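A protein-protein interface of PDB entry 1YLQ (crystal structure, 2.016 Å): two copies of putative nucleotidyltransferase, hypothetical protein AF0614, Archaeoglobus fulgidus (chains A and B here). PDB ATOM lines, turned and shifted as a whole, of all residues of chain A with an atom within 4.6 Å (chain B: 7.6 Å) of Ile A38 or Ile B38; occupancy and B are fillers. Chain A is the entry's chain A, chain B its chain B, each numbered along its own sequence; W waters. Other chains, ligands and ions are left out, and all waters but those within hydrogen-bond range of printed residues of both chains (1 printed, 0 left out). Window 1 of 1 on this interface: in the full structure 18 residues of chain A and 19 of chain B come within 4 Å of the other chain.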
ATOM      1  N   LEU A  22       3.588  33.122 -14.628  1.00  0.00           N
ATOM      2  CA  LEU A  22       3.211  31.693 -14.669  1.00  0.00           C
ATOM      3  C   LEU A  22       1.691  31.532 -14.686  1.00  0.00           C
ATOM      4  O   LEU A  22       0.978  32.219 -13.964  1.00  0.00           O
ATOM      5  CB  LEU A  22       3.811  30.944 -13.453  1.00  0.00           C
ATOM      6  CG  LEU A  22       5.354  30.912 -13.331  1.00  0.00           C
ATOM      7  CD1 LEU A  22       5.812  29.982 -12.112  1.00  0.00           C
ATOM      8  CD2 LEU A  22       5.981  30.404 -14.665  1.00  0.00           C
ATOM      9  N   TYR A  23       1.178  30.672 -15.553  1.00  0.00           N
ATOM     10  CA  TYR A  23      -0.212  30.258 -15.478  1.00  0.00           C
ATOM     11  C   TYR A  23      -0.291  28.815 -15.980  1.00  0.00           C
ATOM     12  O   TYR A  23       0.694  28.050 -15.851  1.00  0.00           O
ATOM     13  CB  TYR A  23      -1.151  31.261 -16.204  1.00  0.00           C
ATOM     14  CG  TYR A  23      -0.745  31.617 -17.616  1.00  0.00           C
ATOM     15  CD1 TYR A  23       0.349  32.457 -17.821  1.00  0.00           C
ATOM     16  CD2 TYR A  23      -1.500  31.185 -18.751  1.00  0.00           C
ATOM     17  CE1 TYR A  23       0.752  32.817 -19.086  1.00  0.00           C
ATOM     18  CE2 TYR A  23      -1.067  31.557 -20.104  1.00  0.00           C
ATOM     19  CZ  TYR A  23       0.063  32.388 -20.196  1.00  0.00           C
ATOM     20  OH  TYR A  23       0.596  32.872 -21.359  1.00  0.00           O
ATOM     21  N   VAL A  26      -1.693  24.239 -13.150  1.00  0.00           N
ATOM     22  CA  VAL A  26      -1.276  24.246 -11.743  1.00  0.00           C
ATOM     23  C   VAL A  26      -1.651  25.553 -11.061  1.00  0.00           C
ATOM     24  O   VAL A  26      -2.297  25.559  -9.992  1.00  0.00           O
ATOM     25  CB  VAL A  26       0.191  23.840 -11.582  1.00  0.00           C
ATOM     26  CG1 VAL A  26       0.618  23.914 -10.089  1.00  0.00           C
ATOM     27  CG2 VAL A  26       0.362  22.393 -12.062  1.00  0.00           C
ATOM     28  N   SER A  36      -2.155  23.789 -20.647  1.00  0.00           N
ATOM     29  CA  SER A  36      -0.786  23.346 -20.387  1.00  0.00           C
ATOM     30  C   SER A  36      -0.463  23.270 -18.867  1.00  0.00           C
ATOM     31  O   SER A  36      -1.008  24.046 -18.097  1.00  0.00           O
ATOM     32  CB  SER A  36       0.201  24.263 -21.091  1.00  0.00           C
ATOM     33  OG  SER A  36       1.514  23.942 -20.648  1.00  0.00           O
ATOM     34  N   ASP A  37       0.436  22.375 -18.454  1.00  0.00           N
ATOM     35  CA  ASP A  37       0.795  22.210 -17.022  1.00  0.00           C
ATOM     36  C   ASP A  37       1.285  23.525 -16.399  1.00  0.00           C
ATOM     37  O   ASP A  37       0.776  23.958 -15.361  1.00  0.00           O
ATOM     38  CB  ASP A  37       1.861  21.134 -16.818  1.00  0.00           C
ATOM     39  CG  ASP A  37       1.381  19.699 -17.231  1.00  0.00           C
ATOM     40  OD1 ASP A  37       0.178  19.430 -17.296  1.00  0.00           O
ATOM     41  OD2 ASP A  37       2.239  18.845 -17.505  1.00  0.00           O
ATOM     42  N   ILE A  38       2.303  24.131 -17.018  1.00  0.00           N
ATOM     43  CA  ILE A  38       2.770  25.454 -16.638  1.00  0.00           C
ATOM     44  C   ILE A  38       2.907  26.235 -17.965  1.00  0.00           C
ATOM     45  O   ILE A  38       3.655  25.831 -18.886  1.00  0.00           O
ATOM     46  CB  ILE A  38       4.103  25.423 -15.848  1.00  0.00           C
ATOM     47  CG1 ILE A  38       3.970  24.568 -14.575  1.00  0.00           C
ATOM     48  CG2 ILE A  38       4.588  26.878 -15.503  1.00  0.00           C
ATOM     49  CD1 ILE A  38       5.352  24.274 -13.895  1.00  0.00           C
ATOM     50  N   ASP A  39       2.118  27.289 -18.100  1.00  0.00           N
ATOM     51  CA  ASP A  39       2.411  28.315 -19.142  1.00  0.00           C
ATOM     52  C   ASP A  39       3.369  29.345 -18.548  1.00  0.00           C
ATOM     53  O   ASP A  39       3.266  29.703 -17.367  1.00  0.00           O
ATOM     54  CB  ASP A  39       1.148  28.991 -19.603  1.00  0.00           C
ATOM     55  CG  ASP A  39       0.243  28.045 -20.344  1.00  0.00           C
ATOM     56  OD1 ASP A  39       0.606  27.666 -21.486  1.00  0.00           O
ATOM     57  OD2 ASP A  39      -0.782  27.614 -19.743  1.00  0.00           O
ATOM     58  N   VAL A  40       4.326  29.769 -19.357  1.00  0.00           N
ATOM     59  CA  VAL A  40       5.332  30.766 -18.952  1.00  0.00           C
ATOM     60  C   VAL A  40       5.294  31.896 -19.962  1.00  0.00           C
ATOM     61  O   VAL A  40       5.696  31.730 -21.113  1.00  0.00           O
ATOM     62  CB  VAL A  40       6.734  30.184 -18.961  1.00  0.00           C
ATOM     63  CG1 VAL A  40       7.732  31.186 -18.322  1.00  0.00           C
ATOM     64  CG2 VAL A  40       6.808  28.874 -18.171  1.00  0.00           C
ATOM     65  N   PRO A  68       7.229  20.186 -19.280  1.00  0.00           N
ATOM     66  CA  PRO A  68       5.857  20.634 -18.971  1.00  0.00           C
ATOM     67  C   PRO A  68       5.591  22.121 -19.220  1.00  0.00           C
ATOM     68  O   PRO A  68       4.427  22.510 -19.175  1.00  0.00           O
ATOM     69  CB  PRO A  68       5.707  20.320 -17.470  1.00  0.00           C
ATOM     70  CG  PRO A  68       7.068  20.417 -16.949  1.00  0.00           C
ATOM     71  CD  PRO A  68       7.979  19.897 -18.043  1.00  0.00           C
ATOM     72  N   PHE A  69       6.643  22.917 -19.479  1.00  0.00           N
ATOM     73  CA  PHE A  69       6.530  24.375 -19.806  1.00  0.00           C
ATOM     74  C   PHE A  69       6.049  24.693 -21.225  1.00  0.00           C
ATOM     75  O   PHE A  69       6.505  24.096 -22.193  1.00  0.00           O
ATOM     76  CB  PHE A  69       7.867  25.117 -19.546  1.00  0.00           C
ATOM     77  CG  PHE A  69       8.425  24.905 -18.145  1.00  0.00           C
ATOM     78  CD1 PHE A  69       7.799  25.431 -17.046  1.00  0.00           C
ATOM     79  CD2 PHE A  69       9.572  24.153 -17.951  1.00  0.00           C
ATOM     80  CE1 PHE A  69       8.334  25.203 -15.740  1.00  0.00           C
ATOM     81  CE2 PHE A  69      10.096  23.912 -16.666  1.00  0.00           C
ATOM     82  CZ  PHE A  69       9.491  24.449 -15.575  1.00  0.00           C
ATOM     83  N   GLU A  70       5.120  25.616 -21.355  1.00  0.00           N
ATOM     84  CA  GLU A  70       4.724  26.133 -22.667  1.00  0.00           C
ATOM     85  C   GLU A  70       5.124  27.589 -22.596  1.00  0.00           C
ATOM     86  O   GLU A  70       4.656  28.283 -21.727  1.00  0.00           O
ATOM     87  CB  GLU A  70       3.201  25.933 -22.930  1.00  0.00           C
ATOM     88  CG  GLU A  70       2.695  26.539 -24.280  1.00  0.00           C
ATOM     89  CD  GLU A  70       1.218  26.215 -24.616  1.00  0.00           C
ATOM     90  OE1 GLU A  70       0.855  25.019 -24.711  1.00  0.00           O
ATOM     91  OE2 GLU A  70       0.428  27.171 -24.876  1.00  0.00           O
ATOM     92  N   ALA B   1       1.678  20.793 -20.295  1.00  0.00           N
ATOM     93  CA  ALA B   1       2.148  20.282 -21.579  1.00  0.00           C
ATOM     94  C   ALA B   1       1.835  18.830 -21.507  1.00  0.00           C
ATOM     95  O   ALA B   1       2.581  17.993 -21.957  1.00  0.00           O
ATOM     96  CB  ALA B   1       3.631  20.505 -21.765  1.00  0.00           C
ATOM     97  N   GLY B   2       0.691  18.532 -20.926  1.00  0.00           N
ATOM     98  CA  GLY B   2       0.213  17.192 -20.924  1.00  0.00           C
ATOM     99  C   GLY B   2       1.095  16.246 -20.114  1.00  0.00           C
ATOM    100  O   GLY B   2       0.835  15.062 -20.195  1.00  0.00           O
ATOM    101  N   MET B   4       1.320  16.046 -16.625  1.00  0.00           N
ATOM    102  CA  MET B   4       0.460  15.614 -15.519  1.00  0.00           C
ATOM    103  C   MET B   4      -0.555  14.542 -15.868  1.00  0.00           C
ATOM    104  O   MET B   4      -0.845  13.677 -15.053  1.00  0.00           O
ATOM    105  CB  MET B   4      -0.254  16.789 -14.938  1.00  0.00           C
ATOM    106  CG  MET B   4       0.717  17.492 -14.096  1.00  0.00           C
ATOM    107  SD  MET B   4       0.096  19.037 -13.596  1.00  0.00           S
ATOM    108  CE  MET B   4       1.634  19.483 -12.781  1.00  0.00           C
ATOM    109  N   ILE B   7       1.428  11.381 -15.932  1.00  0.00           N
ATOM    110  CA  ILE B   7       1.658  10.917 -14.554  1.00  0.00           C
ATOM    111  C   ILE B   7       0.412  10.180 -14.021  1.00  0.00           C
ATOM    112  O   ILE B   7       0.507   9.133 -13.401  1.00  0.00           O
ATOM    113  CB  ILE B   7       2.032  12.132 -13.621  1.00  0.00           C
ATOM    114  CG1 ILE B   7       3.404  12.727 -14.045  1.00  0.00           C
ATOM    115  CG2 ILE B   7       2.064  11.724 -12.122  1.00  0.00           C
ATOM    116  CD1 ILE B   7       3.753  14.062 -13.432  1.00  0.00           C
ATOM    117  N   TYR B  21      -1.134  14.057  -5.150  1.00  0.00           N
ATOM    118  CA  TYR B  21      -1.196  15.374  -4.596  1.00  0.00           C
ATOM    119  C   TYR B  21      -0.050  16.161  -5.165  1.00  0.00           C
ATOM    120  O   TYR B  21       1.086  15.631  -5.279  1.00  0.00           O
ATOM    121  CB  TYR B  21      -1.070  15.290  -3.070  1.00  0.00           C
ATOM    122  CG  TYR B  21      -2.122  14.433  -2.426  1.00  0.00           C
ATOM    123  CD1 TYR B  21      -3.365  14.948  -2.098  1.00  0.00           C
ATOM    124  CD2 TYR B  21      -1.860  13.091  -2.128  1.00  0.00           C
ATOM    125  CE1 TYR B  21      -4.335  14.137  -1.483  1.00  0.00           C
ATOM    126  CE2 TYR B  21      -2.815  12.283  -1.554  1.00  0.00           C
ATOM    127  CZ  TYR B  21      -4.040  12.822  -1.204  1.00  0.00           C
ATOM    128  OH  TYR B  21      -4.978  11.997  -0.622  1.00  0.00           O
ATOM    129  N   LEU B  22      -0.323  17.436  -5.449  1.00  0.00           N
ATOM    130  CA  LEU B  22       0.666  18.383  -6.020  1.00  0.00           C
ATOM    131  C   LEU B  22       1.056  19.428  -4.976  1.00  0.00           C
ATOM    132  O   LEU B  22       0.204  19.936  -4.269  1.00  0.00           O
ATOM    133  CB  LEU B  22       0.081  19.062  -7.278  1.00  0.00           C
ATOM    134  CG  LEU B  22      -0.207  18.179  -8.501  1.00  0.00           C
ATOM    135  CD1 LEU B  22      -0.595  19.061  -9.745  1.00  0.00           C
ATOM    136  CD2 LEU B  22       1.042  17.355  -8.825  1.00  0.00           C
ATOM    137  N   TYR B  23       2.348  19.718  -4.831  1.00  0.00           N
ATOM    138  CA  TYR B  23       2.805  20.884  -4.073  1.00  0.00           C
ATOM    139  C   TYR B  23       4.138  21.342  -4.689  1.00  0.00           C
ATOM    140  O   TYR B  23       4.382  21.114  -5.893  1.00  0.00           O
ATOM    141  CB  TYR B  23       2.858  20.607  -2.552  1.00  0.00           C
ATOM    142  CG  TYR B  23       3.573  19.318  -2.180  1.00  0.00           C
ATOM    143  CD1 TYR B  23       2.990  18.074  -2.460  1.00  0.00           C
ATOM    144  CD2 TYR B  23       4.816  19.350  -1.513  1.00  0.00           C
ATOM    145  CE1 TYR B  23       3.638  16.881  -2.134  1.00  0.00           C
ATOM    146  CE2 TYR B  23       5.488  18.140  -1.169  1.00  0.00           C
ATOM    147  CZ  TYR B  23       4.864  16.931  -1.503  1.00  0.00           C
ATOM    148  OH  TYR B  23       5.459  15.754  -1.176  1.00  0.00           O
ATOM    149  N   GLY B  24       4.972  22.022  -3.922  1.00  0.00           N
ATOM    150  CA  GLY B  24       6.207  22.650  -4.473  1.00  0.00           C
ATOM    151  C   GLY B  24       5.956  24.136  -4.754  1.00  0.00           C
ATOM    152  O   GLY B  24       4.939  24.659  -4.351  1.00  0.00           O
ATOM    153  N   SER B  25       6.874  24.829  -5.406  1.00  0.00           N
ATOM    154  CA  SER B  25       6.832  26.321  -5.378  1.00  0.00           C
ATOM    155  C   SER B  25       5.597  26.908  -6.047  1.00  0.00           C
ATOM    156  O   SER B  25       4.997  27.850  -5.529  1.00  0.00           O
ATOM    157  CB  SER B  25       8.088  26.930  -5.993  1.00  0.00           C
ATOM    158  OG  SER B  25       8.224  26.528  -7.326  1.00  0.00           O
ATOM    159  N   VAL B  26       5.212  26.312  -7.179  1.00  0.00           N
ATOM    160  CA  VAL B  26       4.058  26.796  -7.954  1.00  0.00           C
ATOM    161  C   VAL B  26       2.739  26.756  -7.156  1.00  0.00           C
ATOM    162  O   VAL B  26       1.994  27.760  -7.070  1.00  0.00           O
ATOM    163  CB  VAL B  26       3.965  26.101  -9.306  1.00  0.00           C
ATOM    164  CG1 VAL B  26       2.790  26.724 -10.140  1.00  0.00           C
ATOM    165  CG2 VAL B  26       5.260  26.335 -10.074  1.00  0.00           C
ATOM    166  N   VAL B  27       2.498  25.634  -6.500  1.00  0.00           N
ATOM    167  CA  VAL B  27       1.278  25.451  -5.737  1.00  0.00           C
ATOM    168  C   VAL B  27       1.324  26.296  -4.466  1.00  0.00           C
ATOM    169  O   VAL B  27       0.305  26.932  -4.113  1.00  0.00           O
ATOM    170  CB  VAL B  27       1.054  23.936  -5.405  1.00  0.00           C
ATOM    171  CG1 VAL B  27      -0.065  23.729  -4.318  1.00  0.00           C
ATOM    172  CG2 VAL B  27       0.750  23.142  -6.705  1.00  0.00           C
ATOM    173  N   TYR B  31       8.495  30.787  -4.112  1.00  0.00           N
ATOM    174  CA  TYR B  31       9.511  30.695  -5.146  1.00  0.00           C
ATOM    175  C   TYR B  31      10.866  31.150  -4.622  1.00  0.00           C
ATOM    176  O   TYR B  31      11.818  31.222  -5.393  1.00  0.00           O
ATOM    177  CB  TYR B  31       9.136  31.555  -6.354  1.00  0.00           C
ATOM    178  CG  TYR B  31       7.837  31.190  -6.996  1.00  0.00           C
ATOM    179  CD1 TYR B  31       7.766  30.175  -7.952  1.00  0.00           C
ATOM    180  CD2 TYR B  31       6.668  31.878  -6.673  1.00  0.00           C
ATOM    181  CE1 TYR B  31       6.555  29.863  -8.573  1.00  0.00           C
ATOM    182  CE2 TYR B  31       5.452  31.559  -7.275  1.00  0.00           C
ATOM    183  CZ  TYR B  31       5.400  30.551  -8.216  1.00  0.00           C
ATOM    184  OH  TYR B  31       4.193  30.242  -8.792  1.00  0.00           O
ATOM    185  N   LEU B  35      12.060  25.458  -2.876  1.00  0.00           N
ATOM    186  CA  LEU B  35      11.232  24.258  -3.034  1.00  0.00           C
ATOM    187  C   LEU B  35      11.458  23.721  -4.446  1.00  0.00           C
ATOM    188  O   LEU B  35      11.850  24.487  -5.334  1.00  0.00           O
ATOM    189  CB  LEU B  35       9.745  24.580  -2.859  1.00  0.00           C
ATOM    190  CG  LEU B  35       9.213  25.141  -1.540  1.00  0.00           C
ATOM    191  CD1 LEU B  35       7.678  25.068  -1.542  1.00  0.00           C
ATOM    192  CD2 LEU B  35       9.808  24.390  -0.344  1.00  0.00           C
ATOM    193  N   SER B  36      11.238  22.422  -4.645  1.00  0.00           N
ATOM    194  CA  SER B  36      11.063  21.900  -5.998  1.00  0.00           C
ATOM    195  C   SER B  36       9.922  22.634  -6.749  1.00  0.00           C
ATOM    196  O   SER B  36       8.966  23.041  -6.113  1.00  0.00           O
ATOM    197  CB  SER B  36      10.768  20.411  -5.950  1.00  0.00           C
ATOM    198  OG  SER B  36      10.522  19.958  -7.276  1.00  0.00           O
ATOM    199  N   ASP B  37      10.013  22.772  -8.074  1.00  0.00           N
ATOM    200  CA  ASP B  37       8.977  23.465  -8.887  1.00  0.00           C
ATOM    201  C   ASP B  37       7.580  22.835  -8.698  1.00  0.00           C
ATOM    202  O   ASP B  37       6.610  23.533  -8.357  1.00  0.00           O
ATOM    203  CB  ASP B  37       9.330  23.457 -10.379  1.00  0.00           C
ATOM    204  CG  ASP B  37      10.625  24.267 -10.713  1.00  0.00           C
ATOM    205  OD1 ASP B  37      11.063  25.120  -9.927  1.00  0.00           O
ATOM    206  OD2 ASP B  37      11.202  24.035 -11.785  1.00  0.00           O
ATOM    207  N   ILE B  38       7.500  21.519  -8.937  1.00  0.00           N
ATOM    208  CA  ILE B  38       6.301  20.716  -8.672  1.00  0.00           C
ATOM    209  C   ILE B  38       6.734  19.448  -7.906  1.00  0.00           C
ATOM    210  O   ILE B  38       7.462  18.589  -8.436  1.00  0.00           O
ATOM    211  CB  ILE B  38       5.569  20.333  -9.980  1.00  0.00           C
ATOM    212  CG1 ILE B  38       5.163  21.588 -10.774  1.00  0.00           C
ATOM    213  CG2 ILE B  38       4.309  19.465  -9.693  1.00  0.00           C
ATOM    214  CD1 ILE B  38       4.664  21.252 -12.208  1.00  0.00           C
ATOM    215  N   ASP B  39       6.306  19.344  -6.650  1.00  0.00           N
ATOM    216  CA  ASP B  39       6.355  18.045  -5.919  1.00  0.00           C
ATOM    217  C   ASP B  39       5.102  17.243  -6.228  1.00  0.00           C
ATOM    218  O   ASP B  39       4.014  17.791  -6.321  1.00  0.00           O
ATOM    219  CB  ASP B  39       6.433  18.282  -4.417  1.00  0.00           C
ATOM    220  CG  ASP B  39       7.737  18.922  -4.008  1.00  0.00           C
ATOM    221  OD1 ASP B  39       8.780  18.220  -4.028  1.00  0.00           O
ATOM    222  OD2 ASP B  39       7.714  20.138  -3.704  1.00  0.00           O
ATOM    223  N   VAL B  40       5.269  15.958  -6.440  1.00  0.00           N
ATOM    224  CA  VAL B  40       4.158  15.069  -6.765  1.00  0.00           C
ATOM    225  C   VAL B  40       4.212  13.933  -5.745  1.00  0.00           C
ATOM    226  O   VAL B  40       5.109  13.050  -5.757  1.00  0.00           O
ATOM    227  CB  VAL B  40       4.265  14.485  -8.182  1.00  0.00           C
ATOM    228  CG1 VAL B  40       3.002  13.572  -8.508  1.00  0.00           C
ATOM    229  CG2 VAL B  40       4.384  15.588  -9.263  1.00  0.00           C
ATOM    230  N   ALA B  41       3.251  13.922  -4.855  1.00  0.00           N
ATOM    231  CA  ALA B  41       3.165  12.779  -3.936  1.00  0.00           C
ATOM    232  C   ALA B  41       2.173  11.756  -4.517  1.00  0.00           C
ATOM    233  O   ALA B  41       1.045  12.108  -4.845  1.00  0.00           O
ATOM    234  CB  ALA B  41       2.734  13.234  -2.572  1.00  0.00           C
ATOM    235  N   SER B  67      13.278  16.452 -15.347  1.00  0.00           N
ATOM    236  CA  SER B  67      12.073  17.265 -15.458  1.00  0.00           C
ATOM    237  C   SER B  67      11.861  18.088 -14.188  1.00  0.00           C
ATOM    238  O   SER B  67      12.583  17.904 -13.177  1.00  0.00           O
ATOM    239  CB  SER B  67      10.851  16.410 -15.777  1.00  0.00           C
ATOM    240  OG  SER B  67      10.199  16.015 -14.595  1.00  0.00           O
ATOM    241  N   PRO B  68      10.868  18.984 -14.216  1.00  0.00           N
ATOM    242  CA  PRO B  68      10.663  19.775 -13.014  1.00  0.00           C
ATOM    243  C   PRO B  68       9.936  19.040 -11.884  1.00  0.00           C
ATOM    244  O   PRO B  68       9.889  19.593 -10.803  1.00  0.00           O
ATOM    245  CB  PRO B  68       9.842  20.980 -13.510  1.00  0.00           C
ATOM    246  CG  PRO B  68       9.137  20.500 -14.696  1.00  0.00           C
ATOM    247  CD  PRO B  68       9.897  19.318 -15.273  1.00  0.00           C
ATOM    248  N   PHE B  69       9.411  17.826 -12.126  1.00  0.00           N
ATOM    249  CA  PHE B  69       8.720  16.997 -11.094  1.00  0.00           C
ATOM    250  C   PHE B  69       9.682  16.337 -10.104  1.00  0.00           C
ATOM    251  O   PHE B  69      10.723  15.799 -10.488  1.00  0.00           O
ATOM    252  CB  PHE B  69       7.800  15.915 -11.721  1.00  0.00           C
ATOM    253  CG  PHE B  69       6.800  16.470 -12.730  1.00  0.00           C
ATOM    254  CD1 PHE B  69       5.735  17.253 -12.317  1.00  0.00           C
ATOM    255  CD2 PHE B  69       6.979  16.270 -14.087  1.00  0.00           C
ATOM    256  CE1 PHE B  69       4.825  17.795 -13.290  1.00  0.00           C
ATOM    257  CE2 PHE B  69       6.099  16.814 -15.052  1.00  0.00           C
ATOM    258  CZ  PHE B  69       5.015  17.559 -14.648  1.00  0.00           C
ATOM    259  N   GLU B  70       9.331  16.380  -8.831  1.00  0.00           N
ATOM    260  CA  GLU B  70      10.048  15.617  -7.807  1.00  0.00           C
ATOM    261  C   GLU B  70       9.000  14.706  -7.245  1.00  0.00           C
ATOM    262  O   GLU B  70       7.999  15.184  -6.729  1.00  0.00           O
ATOM    263  CB  GLU B  70      10.617  16.555  -6.721  1.00  0.00           C
ATOM    264  CG  GLU B  70      11.380  15.810  -5.608  1.00  0.00           C
ATOM    265  CD  GLU B  70      12.034  16.744  -4.571  1.00  0.00           C
ATOM    266  OE1 GLU B  70      13.053  17.383  -4.897  1.00  0.00           O
ATOM    267  OE2 GLU B  70      11.561  16.801  -3.413  1.00  0.00           O
ATOM    268  N   PHE B  71       9.208  13.381  -7.384  1.00  0.00           N
ATOM    269  CA  PHE B  71       8.226  12.382  -7.030  1.00  0.00           C
ATOM    270  C   PHE B  71       8.504  11.854  -5.622  1.00  0.00           C
ATOM    271  O   PHE B  71       9.665  11.659  -5.273  1.00  0.00           O
ATOM    272  CB  PHE B  71       8.302  11.199  -8.034  1.00  0.00           C
ATOM    273  CG  PHE B  71       7.863  11.576  -9.415  1.00  0.00           C
ATOM    274  CD1 PHE B  71       6.507  11.666  -9.716  1.00  0.00           C
ATOM    275  CD2 PHE B  71       8.819  11.869 -10.415  1.00  0.00           C
ATOM    276  CE1 PHE B  71       6.066  12.035 -11.023  1.00  0.00           C
ATOM    277  CE2 PHE B  71       8.406  12.255 -11.726  1.00  0.00           C
ATOM    278  CZ  PHE B  71       7.043  12.317 -12.026  1.00  0.00           C
ATOM    279  N   HIS B  72       7.445  11.639  -4.845  1.00  0.00           N
ATOM    280  CA  HIS B  72       7.499  11.049  -3.495  1.00  0.00           C
ATOM    281  C   HIS B  72       6.475   9.945  -3.529  1.00  0.00           C
ATOM    282  O   HIS B  72       5.271  10.213  -3.725  1.00  0.00           O
ATOM    283  CB  HIS B  72       7.160  12.121  -2.448  1.00  0.00           C
ATOM    284  CG  HIS B  72       8.049  13.321  -2.559  1.00  0.00           C
ATOM    285  ND1 HIS B  72       7.722  14.441  -3.307  1.00  0.00           N
ATOM    286  CD2 HIS B  72       9.288  13.542  -2.075  1.00  0.00           C
ATOM    287  CE1 HIS B  72       8.695  15.324  -3.210  1.00  0.00           C
ATOM    288  NE2 HIS B  72       9.678  14.779  -2.520  1.00  0.00           N
HETATM  289  O   HOH W   1      -1.439  17.268 -18.292  1.00  0.00           O
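Ile A38 touches one residue of chain B.
Printed residues of chain B within 4 Å of Pro A68: Ala B1 (3.4 Å) and Pro B68 (3.1 Å).
Of the printed residues of chain A, Met B4 touches Val A26 and Asp A37.
Of the printed residues of chain A, Val B26 touches Val A26.
Of chain A, only Ile A38 (3.5 Å) comes within 4 Å of Ile B38.
The nearest residue of chain B that does not touch Ile A38 is Val B26 (4.3 Å).
The nearest printed residue of chain A that does not touch Tyr B31 is Val A26 (7.4 Å).
Val A26 touches its own counterpart, Val B26.
Ile A38 touches its own counterpart, Ile B38.
Pro B68 touches its own counterpart, Pro A68.
11 positions are printed for both chains.
Water W1 lies within hydrogen-bond range of the side-chain carboxylate (OD1) of Asp A37 and the backbone NH (N) of Met B4.
Among the printed residues, merely in contact across the chains: Pro A68 with Pro B68, Val A26 with Met B4, Val A26 with Val B27, Ile A38 with Ile B38, Val A26 with Val B26, Leu A22 with Tyr B31 and Asp A37 with Gly B2.
Of the 11 printed residues of chain A, 6 touch a printed residue of chain B.
Hydrophobic or aromatic side chains of chain B that line the printed part of chain A: Ala B1, Met B4, Val B26, Val B27, Tyr B31, Ile B38 and Pro B68.
Among the printed residues, no Asp or Glu carboxylate lies within 4 Å of a Lys or Arg side-chain nitrogen of the other chain.
OG of Ser A36 lies within hydrogen-bond range of N of Ala B1 (3.2 Å).
OD2 of Asp A37 sits close to N of Ala B1, at 3.4 Å.
The backbone NH of Met B4 is in hydrogen-bond range of the side-chain carboxylate of Asp A37 (3.1 Å).
N of Ala B1 lies close to O of Pro A68 (3.4 Å).
N of Val A26 lies within hydrogen-bond range of O of Asp A37.
OG of Ser A36 is in hydrogen-bond range of O of Ile A38.
O of Pro A68 is in hydrogen-bond range of N of Ile A38 (3.4 Å).
The backbone NH of Glu A70 lies within hydrogen-bond range of the backbone carbonyl oxygen of Ile A38, at 2.9 Å.
N of Val B26 is in hydrogen-bond range of O of Asp B37 (3.3 Å).
O of Ile B38 is in hydrogen-bond range of N of Glu B70, at 2.9 Å.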
